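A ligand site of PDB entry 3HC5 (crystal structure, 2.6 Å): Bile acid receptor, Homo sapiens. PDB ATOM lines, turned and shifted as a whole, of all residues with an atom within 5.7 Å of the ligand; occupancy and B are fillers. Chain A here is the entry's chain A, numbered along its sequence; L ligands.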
ATOM      1  N   MET A  25      -0.609  16.982  11.605  1.00  0.00           N
ATOM      2  CA  MET A  25      -0.438  18.014  10.573  1.00  0.00           C
ATOM      3  C   MET A  25       1.043  18.427  10.537  1.00  0.00           C
ATOM      4  O   MET A  25       1.591  18.878  11.532  1.00  0.00           O
ATOM      5  CB  MET A  25      -1.287  19.254  10.915  1.00  0.00           C
ATOM      6  CG  MET A  25      -2.796  19.054  10.892  1.00  0.00           C
ATOM      7  SD  MET A  25      -3.546  19.201   9.254  1.00  0.00           S
ATOM      8  CE  MET A  25      -3.674  20.964   9.091  1.00  0.00           C
ATOM      9  N   THR A  30       1.362  23.563   7.900  1.00  0.00           N
ATOM     10  CA  THR A  30       0.642  24.587   8.646  1.00  0.00           C
ATOM     11  C   THR A  30       1.422  25.900   8.662  1.00  0.00           C
ATOM     12  O   THR A  30       0.840  26.959   8.942  1.00  0.00           O
ATOM     13  CB  THR A  30       0.302  24.123  10.089  1.00  0.00           C
ATOM     14  OG1 THR A  30       1.499  23.842  10.817  1.00  0.00           O
ATOM     15  CG2 THR A  30      -0.530  22.872  10.046  1.00  0.00           C
ATOM     16  N   ILE A  33       0.187  29.033   6.622  1.00  0.00           N
ATOM     17  CA  ILE A  33      -0.820  29.947   7.131  1.00  0.00           C
ATOM     18  C   ILE A  33      -0.155  31.279   7.443  1.00  0.00           C
ATOM     19  O   ILE A  33      -0.741  32.346   7.269  1.00  0.00           O
ATOM     20  CB  ILE A  33      -1.455  29.386   8.383  1.00  0.00           C
ATOM     21  CG1 ILE A  33      -2.362  28.208   8.023  1.00  0.00           C
ATOM     22  CG2 ILE A  33      -2.193  30.475   9.112  1.00  0.00           C
ATOM     23  CD1 ILE A  33      -2.762  27.351   9.211  1.00  0.00           C
ATOM     24  N   PHE A  44      -7.915  30.991   0.245  1.00  0.00           N
ATOM     25  CA  PHE A  44      -8.794  29.856  -0.027  1.00  0.00           C
ATOM     26  C   PHE A  44      -8.052  28.568  -0.315  1.00  0.00           C
ATOM     27  O   PHE A  44      -8.469  27.512   0.146  1.00  0.00           O
ATOM     28  CB  PHE A  44      -9.735  30.159  -1.192  1.00  0.00           C
ATOM     29  CG  PHE A  44     -10.616  29.003  -1.553  1.00  0.00           C
ATOM     30  CD1 PHE A  44     -10.197  28.035  -2.459  1.00  0.00           C
ATOM     31  CD2 PHE A  44     -11.860  28.852  -0.939  1.00  0.00           C
ATOM     32  CE1 PHE A  44     -10.984  26.942  -2.747  1.00  0.00           C
ATOM     33  CE2 PHE A  44     -12.679  27.752  -1.223  1.00  0.00           C
ATOM     34  CZ  PHE A  44     -12.238  26.793  -2.131  1.00  0.00           C
ATOM     35  N   LEU A  47      -6.625  27.250   2.993  1.00  0.00           N
ATOM     36  CA  LEU A  47      -7.669  26.718   3.846  1.00  0.00           C
ATOM     37  C   LEU A  47      -8.139  25.357   3.331  1.00  0.00           C
ATOM     38  O   LEU A  47      -8.549  24.499   4.101  1.00  0.00           O
ATOM     39  CB  LEU A  47      -8.846  27.705   3.930  1.00  0.00           C
ATOM     40  CG  LEU A  47      -8.621  28.954   4.786  1.00  0.00           C
ATOM     41  CD1 LEU A  47      -9.767  29.935   4.611  1.00  0.00           C
ATOM     42  CD2 LEU A  47      -8.460  28.556   6.230  1.00  0.00           C
ATOM     43  N   THR A  48      -8.082  25.165   2.015  1.00  0.00           N
ATOM     44  CA  THR A  48      -8.481  23.905   1.409  1.00  0.00           C
ATOM     45  C   THR A  48      -7.435  22.854   1.757  1.00  0.00           C
ATOM     46  O   THR A  48      -7.756  21.699   2.043  1.00  0.00           O
ATOM     47  CB  THR A  48      -8.620  24.026  -0.135  1.00  0.00           C
ATOM     48  OG1 THR A  48      -9.735  24.872  -0.457  1.00  0.00           O
ATOM     49  CG2 THR A  48      -8.868  22.664  -0.751  1.00  0.00           C
ATOM     50  N   MET A  50      -5.438  22.851   4.450  1.00  0.00           N
ATOM     51  CA  MET A  50      -5.489  22.545   5.868  1.00  0.00           C
ATOM     52  C   MET A  50      -6.624  21.546   6.084  1.00  0.00           C
ATOM     53  O   MET A  50      -6.443  20.531   6.750  1.00  0.00           O
ATOM     54  CB  MET A  50      -5.783  23.802   6.701  1.00  0.00           C
ATOM     55  CG  MET A  50      -4.584  24.686   7.117  1.00  0.00           C
ATOM     56  SD  MET A  50      -2.926  24.017   6.914  1.00  0.00           S
ATOM     57  CE  MET A  50      -2.533  24.680   5.310  1.00  0.00           C
ATOM     58  N   ALA A  51      -7.786  21.847   5.511  1.00  0.00           N
ATOM     59  CA  ALA A  51      -8.958  20.969   5.649  1.00  0.00           C
ATOM     60  C   ALA A  51      -8.781  19.567   5.053  1.00  0.00           C
ATOM     61  O   ALA A  51      -9.187  18.569   5.650  1.00  0.00           O
ATOM     62  CB  ALA A  51     -10.179  21.638   5.029  1.00  0.00           C
ATOM     63  N   HIS A  54      -6.575  17.827   7.329  1.00  0.00           N
ATOM     64  CA  HIS A  54      -7.227  17.557   8.589  1.00  0.00           C
ATOM     65  C   HIS A  54      -8.127  16.330   8.489  1.00  0.00           C
ATOM     66  O   HIS A  54      -8.269  15.585   9.448  1.00  0.00           O
ATOM     67  CB  HIS A  54      -8.049  18.771   9.046  1.00  0.00           C
ATOM     68  CG  HIS A  54      -8.520  18.672  10.460  1.00  0.00           C
ATOM     69  ND1 HIS A  54      -7.659  18.614  11.535  1.00  0.00           N
ATOM     70  CD2 HIS A  54      -9.769  18.575  10.981  1.00  0.00           C
ATOM     71  CE1 HIS A  54      -8.355  18.481  12.656  1.00  0.00           C
ATOM     72  NE2 HIS A  54      -9.635  18.459  12.339  1.00  0.00           N
ATOM     73  N   ALA A  84     -17.668  15.317  10.082  1.00  0.00           N
ATOM     74  CA  ALA A  84     -16.596  16.052   9.420  1.00  0.00           C
ATOM     75  C   ALA A  84     -16.566  17.542   9.720  1.00  0.00           C
ATOM     76  O   ALA A  84     -15.584  18.062  10.264  1.00  0.00           O
ATOM     77  CB  ALA A  84     -16.667  15.824   7.931  1.00  0.00           C
ATOM     78  N   VAL A  85     -17.645  18.243   9.350  1.00  0.00           N
ATOM     79  CA  VAL A  85     -17.741  19.672   9.575  1.00  0.00           C
ATOM     80  C   VAL A  85     -17.630  20.069  11.038  1.00  0.00           C
ATOM     81  O   VAL A  85     -16.823  20.914  11.388  1.00  0.00           O
ATOM     82  CB  VAL A  85     -19.053  20.237   9.006  1.00  0.00           C
ATOM     83  CG1 VAL A  85     -19.328  21.610   9.570  1.00  0.00           C
ATOM     84  CG2 VAL A  85     -18.951  20.324   7.497  1.00  0.00           C
ATOM     85  N   MET A  88     -14.288  19.759  12.530  1.00  0.00           N
ATOM     86  CA  MET A  88     -13.399  20.776  12.002  1.00  0.00           C
ATOM     87  C   MET A  88     -13.618  22.107  12.696  1.00  0.00           C
ATOM     88  O   MET A  88     -12.682  22.863  12.905  1.00  0.00           O
ATOM     89  CB  MET A  88     -13.589  20.916  10.490  1.00  0.00           C
ATOM     90  CG  MET A  88     -13.032  19.751   9.693  1.00  0.00           C
ATOM     91  SD  MET A  88     -13.321  19.858   7.889  1.00  0.00           S
ATOM     92  CE  MET A  88     -12.534  18.364   7.305  1.00  0.00           C
ATOM     93  N   PHE A  89     -14.871  22.396  13.055  1.00  0.00           N
ATOM     94  CA  PHE A  89     -15.161  23.641  13.762  1.00  0.00           C
ATOM     95  C   PHE A  89     -14.570  23.556  15.152  1.00  0.00           C
ATOM     96  O   PHE A  89     -14.125  24.550  15.705  1.00  0.00           O
ATOM     97  CB  PHE A  89     -16.656  23.875  13.878  1.00  0.00           C
ATOM     98  CG  PHE A  89     -17.191  24.789  12.835  1.00  0.00           C
ATOM     99  CD1 PHE A  89     -17.794  24.279  11.696  1.00  0.00           C
ATOM    100  CD2 PHE A  89     -17.083  26.160  12.997  1.00  0.00           C
ATOM    101  CE1 PHE A  89     -18.283  25.123  10.716  1.00  0.00           C
ATOM    102  CE2 PHE A  89     -17.568  27.018  12.018  1.00  0.00           C
ATOM    103  CZ  PHE A  89     -18.162  26.497  10.883  1.00  0.00           C
ATOM    104  N   ARG A  91     -11.858  21.873  16.031  1.00  0.00           N
ATOM    105  CA  ARG A  91     -10.405  22.018  15.947  1.00  0.00           C
ATOM    106  C   ARG A  91      -9.991  23.471  15.738  1.00  0.00           C
ATOM    107  O   ARG A  91      -9.078  23.962  16.398  1.00  0.00           O
ATOM    108  CB  ARG A  91      -9.832  21.152  14.835  1.00  0.00           C
ATOM    109  CG  ARG A  91      -8.301  21.151  14.804  1.00  0.00           C
ATOM    110  CD  ARG A  91      -7.707  20.881  16.189  1.00  0.00           C
ATOM    111  NE  ARG A  91      -6.252  20.808  16.139  1.00  0.00           N
ATOM    112  CZ  ARG A  91      -5.471  20.510  17.178  1.00  0.00           C
ATOM    113  NH1 ARG A  91      -5.994  20.262  18.370  1.00  0.00           N
ATOM    114  NH2 ARG A  91      -4.155  20.435  17.013  1.00  0.00           N
ATOM    115  N   SER A  92     -10.664  24.161  14.831  1.00  0.00           N
ATOM    116  CA  SER A  92     -10.308  25.545  14.579  1.00  0.00           C
ATOM    117  C   SER A  92     -10.638  26.360  15.818  1.00  0.00           C
ATOM    118  O   SER A  92      -9.857  27.231  16.212  1.00  0.00           O
ATOM    119  CB  SER A  92     -11.043  26.084  13.349  1.00  0.00           C
ATOM    120  OG  SER A  92     -12.435  25.838  13.394  1.00  0.00           O
ATOM    121  N   ILE A  95      -7.954  26.293  18.021  1.00  0.00           N
ATOM    122  CA  ILE A  95      -6.837  27.110  17.530  1.00  0.00           C
ATOM    123  C   ILE A  95      -7.017  28.571  17.976  1.00  0.00           C
ATOM    124  O   ILE A  95      -6.075  29.206  18.434  1.00  0.00           O
ATOM    125  CB  ILE A  95      -6.761  27.127  15.980  1.00  0.00           C
ATOM    126  CG1 ILE A  95      -6.612  25.715  15.416  1.00  0.00           C
ATOM    127  CG2 ILE A  95      -5.619  28.025  15.561  1.00  0.00           C
ATOM    128  CD1 ILE A  95      -5.232  25.145  15.539  1.00  0.00           C
ATOM    129  N   LEU A 100      -3.223  27.770  19.795  1.00  0.00           N
ATOM    130  CA  LEU A 100      -2.210  26.752  19.509  1.00  0.00           C
ATOM    131  C   LEU A 100      -1.208  27.327  18.496  1.00  0.00           C
ATOM    132  O   LEU A 100      -1.580  27.836  17.434  1.00  0.00           O
ATOM    133  CB  LEU A 100      -2.879  25.493  18.918  1.00  0.00           C
ATOM    134  CG  LEU A 100      -4.175  24.934  19.548  1.00  0.00           C
ATOM    135  CD1 LEU A 100      -4.629  23.730  18.749  1.00  0.00           C
ATOM    136  CD2 LEU A 100      -3.959  24.543  20.991  1.00  0.00           C
ATOM    137  N   SER A 102       0.790  26.014  16.244  1.00  0.00           N
ATOM    138  CA  SER A 102       0.710  25.434  14.909  1.00  0.00           C
ATOM    139  C   SER A 102      -0.441  26.035  14.103  1.00  0.00           C
ATOM    140  O   SER A 102      -0.520  25.849  12.889  1.00  0.00           O
ATOM    141  CB  SER A 102       0.531  23.919  15.006  1.00  0.00           C
ATOM    142  N   GLY A 103      -1.328  26.751  14.781  1.00  0.00           N
ATOM    143  CA  GLY A 103      -2.461  27.329  14.091  1.00  0.00           C
ATOM    144  C   GLY A 103      -2.279  28.736  13.574  1.00  0.00           C
ATOM    145  O   GLY A 103      -2.984  29.156  12.648  1.00  0.00           O
ATOM    146  N   HIS A 104      -1.345  29.479  14.165  1.00  0.00           N
ATOM    147  CA  HIS A 104      -1.137  30.850  13.718  1.00  0.00           C
ATOM    148  C   HIS A 104      -2.487  31.553  13.731  1.00  0.00           C
ATOM    149  O   HIS A 104      -2.919  32.139  12.741  1.00  0.00           O
ATOM    150  CB  HIS A 104      -0.520  30.847  12.323  1.00  0.00           C
ATOM    151  CG  HIS A 104       0.692  29.969  12.220  1.00  0.00           C
ATOM    152  ND1 HIS A 104       0.619  28.646  11.849  1.00  0.00           N
ATOM    153  CD2 HIS A 104       1.978  30.194  12.565  1.00  0.00           C
ATOM    154  CE1 HIS A 104       1.813  28.091  11.968  1.00  0.00           C
ATOM    155  NE2 HIS A 104       2.654  29.008  12.396  1.00  0.00           N
ATOM    156  N   LEU A 108      -4.723  32.856  10.719  1.00  0.00           N
ATOM    157  CA  LEU A 108      -5.684  31.890  10.231  1.00  0.00           C
ATOM    158  C   LEU A 108      -6.976  32.680  10.103  1.00  0.00           C
ATOM    159  O   LEU A 108      -7.706  32.566   9.120  1.00  0.00           O
ATOM    160  CB  LEU A 108      -5.856  30.730  11.216  1.00  0.00           C
ATOM    161  CG  LEU A 108      -6.849  29.617  10.814  1.00  0.00           C
ATOM    162  CD1 LEU A 108      -6.333  28.842   9.615  1.00  0.00           C
ATOM    163  CD2 LEU A 108      -7.075  28.676  11.982  1.00  0.00           C
ATOM    164  N   ILE A 112      -9.605  33.282   6.780  1.00  0.00           N
ATOM    165  CA  ILE A 112     -10.994  32.831   6.796  1.00  0.00           C
ATOM    166  C   ILE A 112     -11.908  34.024   6.498  1.00  0.00           C
ATOM    167  O   ILE A 112     -12.933  33.893   5.806  1.00  0.00           O
ATOM    168  CB  ILE A 112     -11.374  32.222   8.181  1.00  0.00           C
ATOM    169  CG1 ILE A 112     -10.736  30.847   8.332  1.00  0.00           C
ATOM    170  CG2 ILE A 112     -12.888  32.146   8.343  1.00  0.00           C
ATOM    171  CD1 ILE A 112     -11.133  30.164   9.623  1.00  0.00           C
ATOM    172  N   ILE A 117     -16.175  33.770   1.842  1.00  0.00           N
ATOM    173  CA  ILE A 117     -17.296  33.420   2.704  1.00  0.00           C
ATOM    174  C   ILE A 117     -18.156  34.661   2.983  1.00  0.00           C
ATOM    175  O   ILE A 117     -17.644  35.725   3.311  1.00  0.00           O
ATOM    176  CB  ILE A 117     -16.836  32.858   4.062  1.00  0.00           C
ATOM    177  CG1 ILE A 117     -15.928  31.654   3.868  1.00  0.00           C
ATOM    178  CG2 ILE A 117     -18.037  32.439   4.877  1.00  0.00           C
ATOM    179  CD1 ILE A 117     -15.283  31.164   5.163  1.00  0.00           C
ATOM    180  N   MET A 125     -20.169  32.122  12.741  1.00  0.00           N
ATOM    181  CA  MET A 125     -18.946  31.372  12.893  1.00  0.00           C
ATOM    182  C   MET A 125     -18.075  31.956  14.014  1.00  0.00           C
ATOM    183  O   MET A 125     -17.761  31.259  14.978  1.00  0.00           O
ATOM    184  CB  MET A 125     -18.201  31.408  11.563  1.00  0.00           C
ATOM    185  CG  MET A 125     -17.060  30.426  11.449  1.00  0.00           C
ATOM    186  SD  MET A 125     -16.403  30.477   9.759  1.00  0.00           S
ATOM    187  CE  MET A 125     -17.933  30.370   8.827  1.00  0.00           C
ATOM    188  N   TYR A 129     -17.064  30.821  17.957  1.00  0.00           N
ATOM    189  CA  TYR A 129     -15.711  30.696  18.516  1.00  0.00           C
ATOM    190  C   TYR A 129     -15.533  31.464  19.826  1.00  0.00           C
ATOM    191  O   TYR A 129     -14.896  30.973  20.767  1.00  0.00           O
ATOM    192  CB  TYR A 129     -14.658  31.174  17.517  1.00  0.00           C
ATOM    193  CG  TYR A 129     -14.516  30.339  16.262  1.00  0.00           C
ATOM    194  CD1 TYR A 129     -14.470  28.949  16.318  1.00  0.00           C
ATOM    195  CD2 TYR A 129     -14.370  30.948  15.023  1.00  0.00           C
ATOM    196  CE1 TYR A 129     -14.285  28.195  15.169  1.00  0.00           C
ATOM    197  CE2 TYR A 129     -14.182  30.209  13.875  1.00  0.00           C
ATOM    198  CZ  TYR A 129     -14.139  28.832  13.949  1.00  0.00           C
ATOM    199  OH  TYR A 129     -13.916  28.104  12.804  1.00  0.00           O
ATOM    200  N   HIS A 207     -22.495  25.374   6.246  1.00  0.00           N
ATOM    201  CA  HIS A 207     -21.403  24.848   5.446  1.00  0.00           C
ATOM    202  C   HIS A 207     -21.866  24.366   4.071  1.00  0.00           C
ATOM    203  O   HIS A 207     -21.115  24.432   3.098  1.00  0.00           O
ATOM    204  CB  HIS A 207     -20.685  23.734   6.184  1.00  0.00           C
ATOM    205  CG  HIS A 207     -19.371  23.377   5.589  1.00  0.00           C
ATOM    206  ND1 HIS A 207     -19.230  22.388   4.638  1.00  0.00           N
ATOM    207  CD2 HIS A 207     -18.151  23.933   5.745  1.00  0.00           C
ATOM    208  CE1 HIS A 207     -17.961  22.349   4.239  1.00  0.00           C
ATOM    209  NE2 HIS A 207     -17.291  23.278   4.899  1.00  0.00           N
ATOM    210  N   MET A 210     -22.063  27.451   2.022  1.00  0.00           N
ATOM    211  CA  MET A 210     -20.742  27.998   1.749  1.00  0.00           C
ATOM    212  C   MET A 210     -20.105  27.251   0.586  1.00  0.00           C
ATOM    213  O   MET A 210     -19.436  27.858  -0.239  1.00  0.00           O
ATOM    214  CB  MET A 210     -19.861  27.889   2.987  1.00  0.00           C
ATOM    215  CG  MET A 210     -20.189  28.910   4.067  1.00  0.00           C
ATOM    216  SD  MET A 210     -19.558  28.473   5.697  1.00  0.00           S
ATOM    217  CE  MET A 210     -17.799  28.298   5.352  1.00  0.00           C
ATOM    218  N   LEU A 211     -20.334  25.941   0.531  1.00  0.00           N
ATOM    219  CA  LEU A 211     -19.794  25.109  -0.527  1.00  0.00           C
ATOM    220  C   LEU A 211     -20.460  25.433  -1.871  1.00  0.00           C
ATOM    221  O   LEU A 211     -19.816  25.388  -2.914  1.00  0.00           O
ATOM    222  CB  LEU A 211     -20.011  23.633  -0.195  1.00  0.00           C
ATOM    223  CG  LEU A 211     -19.270  23.058   1.007  1.00  0.00           C
ATOM    224  CD1 LEU A 211     -19.511  21.579   1.061  1.00  0.00           C
ATOM    225  CD2 LEU A 211     -17.786  23.336   0.901  1.00  0.00           C
ATOM    226  N   TRP A 214     -18.953  28.782  -3.058  1.00  0.00           N
ATOM    227  CA  TRP A 214     -17.619  28.530  -3.584  1.00  0.00           C
ATOM    228  C   TRP A 214     -17.692  27.824  -4.930  1.00  0.00           C
ATOM    229  O   TRP A 214     -17.012  28.203  -5.876  1.00  0.00           O
ATOM    230  CB  TRP A 214     -16.797  27.693  -2.584  1.00  0.00           C
ATOM    231  CG  TRP A 214     -16.215  28.507  -1.471  1.00  0.00           C
ATOM    232  CD1 TRP A 214     -15.576  29.703  -1.585  1.00  0.00           C
ATOM    233  CD2 TRP A 214     -16.103  28.129  -0.089  1.00  0.00           C
ATOM    234  NE1 TRP A 214     -15.074  30.093  -0.367  1.00  0.00           N
ATOM    235  CE2 TRP A 214     -15.390  29.141   0.569  1.00  0.00           C
ATOM    236  CE3 TRP A 214     -16.549  27.032   0.653  1.00  0.00           C
ATOM    237  CZ2 TRP A 214     -15.100  29.099   1.926  1.00  0.00           C
ATOM    238  CZ3 TRP A 214     -16.259  26.982   2.016  1.00  0.00           C
ATOM    239  CH2 TRP A 214     -15.540  28.011   2.632  1.00  0.00           C
ATOM    240  N   PHE A 221     -11.851  21.968  -4.721  1.00  0.00           N
ATOM    241  CA  PHE A 221     -11.635  21.361  -3.417  1.00  0.00           C
ATOM    242  C   PHE A 221     -10.671  20.222  -3.683  1.00  0.00           C
ATOM    243  O   PHE A 221      -9.734  20.373  -4.464  1.00  0.00           O
ATOM    244  CB  PHE A 221     -12.969  20.883  -2.821  1.00  0.00           C
ATOM    245  CG  PHE A 221     -13.910  22.007  -2.473  1.00  0.00           C
ATOM    246  CD1 PHE A 221     -15.094  22.177  -3.148  1.00  0.00           C
ATOM    247  CD2 PHE A 221     -13.568  22.923  -1.488  1.00  0.00           C
ATOM    248  CE1 PHE A 221     -15.924  23.246  -2.855  1.00  0.00           C
ATOM    249  CE2 PHE A 221     -14.398  23.992  -1.195  1.00  0.00           C
ATOM    250  CZ  PHE A 221     -15.580  24.140  -1.880  1.00  0.00           C
ATOM    251  N   LEU A 225     -11.938  15.891   0.118  1.00  0.00           N
ATOM    252  CA  LEU A 225     -12.980  16.742   0.689  1.00  0.00           C
ATOM    253  C   LEU A 225     -14.315  16.513  -0.003  1.00  0.00           C
ATOM    254  O   LEU A 225     -15.360  16.450   0.648  1.00  0.00           O
ATOM    255  CB  LEU A 225     -12.595  18.225   0.561  1.00  0.00           C
ATOM    256  CG  LEU A 225     -11.354  18.679   1.329  1.00  0.00           C
ATOM    257  CD1 LEU A 225     -11.072  20.153   1.065  1.00  0.00           C
ATOM    258  CD2 LEU A 225     -11.571  18.450   2.822  1.00  0.00           C
ATOM    259  N   TRP A 229     -17.628  15.418   1.990  1.00  0.00           N
ATOM    260  CA  TRP A 229     -18.707  16.407   2.087  1.00  0.00           C
ATOM    261  C   TRP A 229     -19.772  16.213   1.009  1.00  0.00           C
ATOM    262  O   TRP A 229     -20.682  17.021   0.873  1.00  0.00           O
ATOM    263  CB  TRP A 229     -18.172  17.854   1.967  1.00  0.00           C
ATOM    264  CG  TRP A 229     -17.348  18.335   3.146  1.00  0.00           C
ATOM    265  CD1 TRP A 229     -17.406  17.866   4.427  1.00  0.00           C
ATOM    266  CD2 TRP A 229     -16.359  19.377   3.141  1.00  0.00           C
ATOM    267  NE1 TRP A 229     -16.507  18.562   5.226  1.00  0.00           N
ATOM    268  CE2 TRP A 229     -15.868  19.489   4.458  1.00  0.00           C
ATOM    269  CE3 TRP A 229     -15.858  20.231   2.153  1.00  0.00           C
ATOM    270  CZ2 TRP A 229     -14.882  20.417   4.806  1.00  0.00           C
ATOM    271  CZ3 TRP A 229     -14.893  21.158   2.498  1.00  0.00           C
ATOM    272  CH2 TRP A 229     -14.410  21.234   3.819  1.00  0.00           C
HETATM  273  C1  LIG L   1     -14.181  26.730   8.147  1.00  0.00           C
HETATM  274  C2  LIG L   1     -14.451  26.813   9.540  1.00  0.00           C
HETATM  275  C3  LIG L   1     -14.863  25.685  10.279  1.00  0.00           C
HETATM  276  C4  LIG L   1     -15.051  24.465   9.623  1.00  0.00           C
HETATM  277  C5  LIG L   1     -14.790  24.340   8.240  1.00  0.00           C
HETATM  278  C6  LIG L   1     -10.484  23.679   7.950  1.00  0.00           C
HETATM  279  C7  LIG L   1     -10.543  22.387   8.514  1.00  0.00           C
HETATM  280  C8  LIG L   1      -9.544  21.954   9.398  1.00  0.00           C
HETATM  281  C9  LIG L   1      -9.429  24.560   8.280  1.00  0.00           C
HETATM  282  C10 LIG L   1      -8.422  24.109   9.174  1.00  0.00           C
HETATM  283  C11 LIG L   1      -8.480  22.825   9.732  1.00  0.00           C
HETATM  284  C12 LIG L   1      -7.384  22.553  10.573  1.00  0.00           C
HETATM  285  C13 LIG L   1      -6.496  23.614  10.674  1.00  0.00           C
HETATM  286  C14 LIG L   1      -4.292  24.598  11.245  1.00  0.00           C
HETATM  287  C15 LIG L   1      -3.064  24.568  11.954  1.00  0.00           C
HETATM  288  C16 LIG L   1     -11.522  25.159   6.331  1.00  0.00           C
HETATM  289  C17 LIG L   1     -12.782  25.206   5.543  1.00  0.00           C
HETATM  290  C18 LIG L   1     -14.070  25.348   6.082  1.00  0.00           C
HETATM  291  N1  LIG L   1     -14.921  25.343   5.090  1.00  0.00           N
HETATM  292  O1  LIG L   1     -14.250  25.204   3.885  1.00  0.00           O
HETATM  293  C19 LIG L   1     -12.932  25.115   4.166  1.00  0.00           C
HETATM  294  C20 LIG L   1     -14.364  25.479   7.500  1.00  0.00           C
HETATM  295  C21 LIG L   1     -11.853  24.963   3.123  1.00  0.00           C
HETATM  296  C22 LIG L   1     -12.131  23.783   2.170  1.00  0.00           C
HETATM  297  C23 LIG L   1     -11.684  26.282   2.335  1.00  0.00           C
HETATM  298 CL1  LIG L   1     -15.039  22.783   7.510  1.00  0.00          CL
HETATM  299 CL2  LIG L   1     -13.668  28.196   7.360  1.00  0.00          CL
HETATM  300  O2  LIG L   1     -11.451  23.992   7.065  1.00  0.00           O
HETATM  301  S1  LIG L   1      -7.053  24.940   9.722  1.00  0.00           S
HETATM  302  C24 LIG L   1      -5.251  23.583  11.416  1.00  0.00           C
HETATM  303  C25 LIG L   1      -2.810  23.496  12.846  1.00  0.00           C
HETATM  304  C26 LIG L   1      -3.764  22.457  13.019  1.00  0.00           C
HETATM  305  C27 LIG L   1      -4.978  22.506  12.304  1.00  0.00           C
HETATM  306  C28 LIG L   1      -3.497  21.351  13.919  1.00  0.00           C
HETATM  307  O3  LIG L   1      -2.446  21.284  14.528  1.00  0.00           O
HETATM  308  O4  LIG L   1      -4.418  20.354  14.100  1.00  0.00           O
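NE of Arg 91 is in salt-bridge range of O4 of the ligand, at 2.8 Å. NE2 of His 207 lies within hydrogen-bond range of N1 of the ligand, at 3.1 Å.
The side-chain hydroxyl (OG) of Ser 92 lies within hydrogen-bond range of the backbone carbonyl oxygen (O) of Met 88 (3.0 Å). The backbone carbonyl oxygen (O) of Ile 95 is in hydrogen-bond range of the backbone NH (N) of Leu 100, at 3.5 Å. The backbone carbonyl oxygen (O) of Thr 30 sits at hydrogen-bond distance from a ring nitrogen (ND1) of His 104 (3.4 Å). The side-chain hydroxyl of Ser 92 is in hydrogen-bond range of the side-chain hydroxyl of Tyr 129, 2.8 Å away. The side-chain hydroxyl (OG1) of Thr 48 lies within hydrogen-bond range of the backbone carbonyl oxygen (O) of Phe 44. O of Ser 102 is in hydrogen-bond range of ND1 of His 104, 3.2 Å away. O of Phe 89 sits at hydrogen-bond distance from OG of Ser 92 (3.1 Å).
Met 25 touches the ligand (CE to C27, 3.8 Å). CG2 of Thr 30 touches C15 of the ligand (3.6 Å). Ile 33 touches the ligand. Phe 44 touches the ligand. Leu 47 touches the ligand (O to C21, 3.5 Å). Thr 48 touches the ligand. CB of Met 50 touches S1 of the ligand, 3.5 Å away. CB of Ala 51 touches O2 of the ligand, 3.4 Å away. His 54 touches the ligand (CB to C8, 3.5 Å). Met 88 touches the ligand. Phe 89 touches the ligand. OG of Ser 92 touches C3 of the ligand, 3.95 Å away. CD1 of Ile 95 touches C26 of the ligand (3.97 Å). Ser 102 touches the ligand. Gly 103 touches the ligand. Leu 108 touches the ligand (CD1 to S1, 3.97 Å). Ile 112 touches the ligand. Tyr 129 touches the ligand. Trp 214 touches the ligand (CZ3 to O1, 3.3 Å). Leu 225 touches the ligand (CD1 to C22, 3.9 Å). CZ2 of Trp 229 touches CL1 of the ligand, at 3.6 Å. Hydrophobic or aromatic side chains within 4 Å of the ligand: Met 25, Ile 33, Phe 44, Leu 47, Met 50, Ala 51, His 54, Met 88, Phe 89, Ile 95, Leu 108, Ile 112, His 207, Trp 214, Leu 225 and Trp 229.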
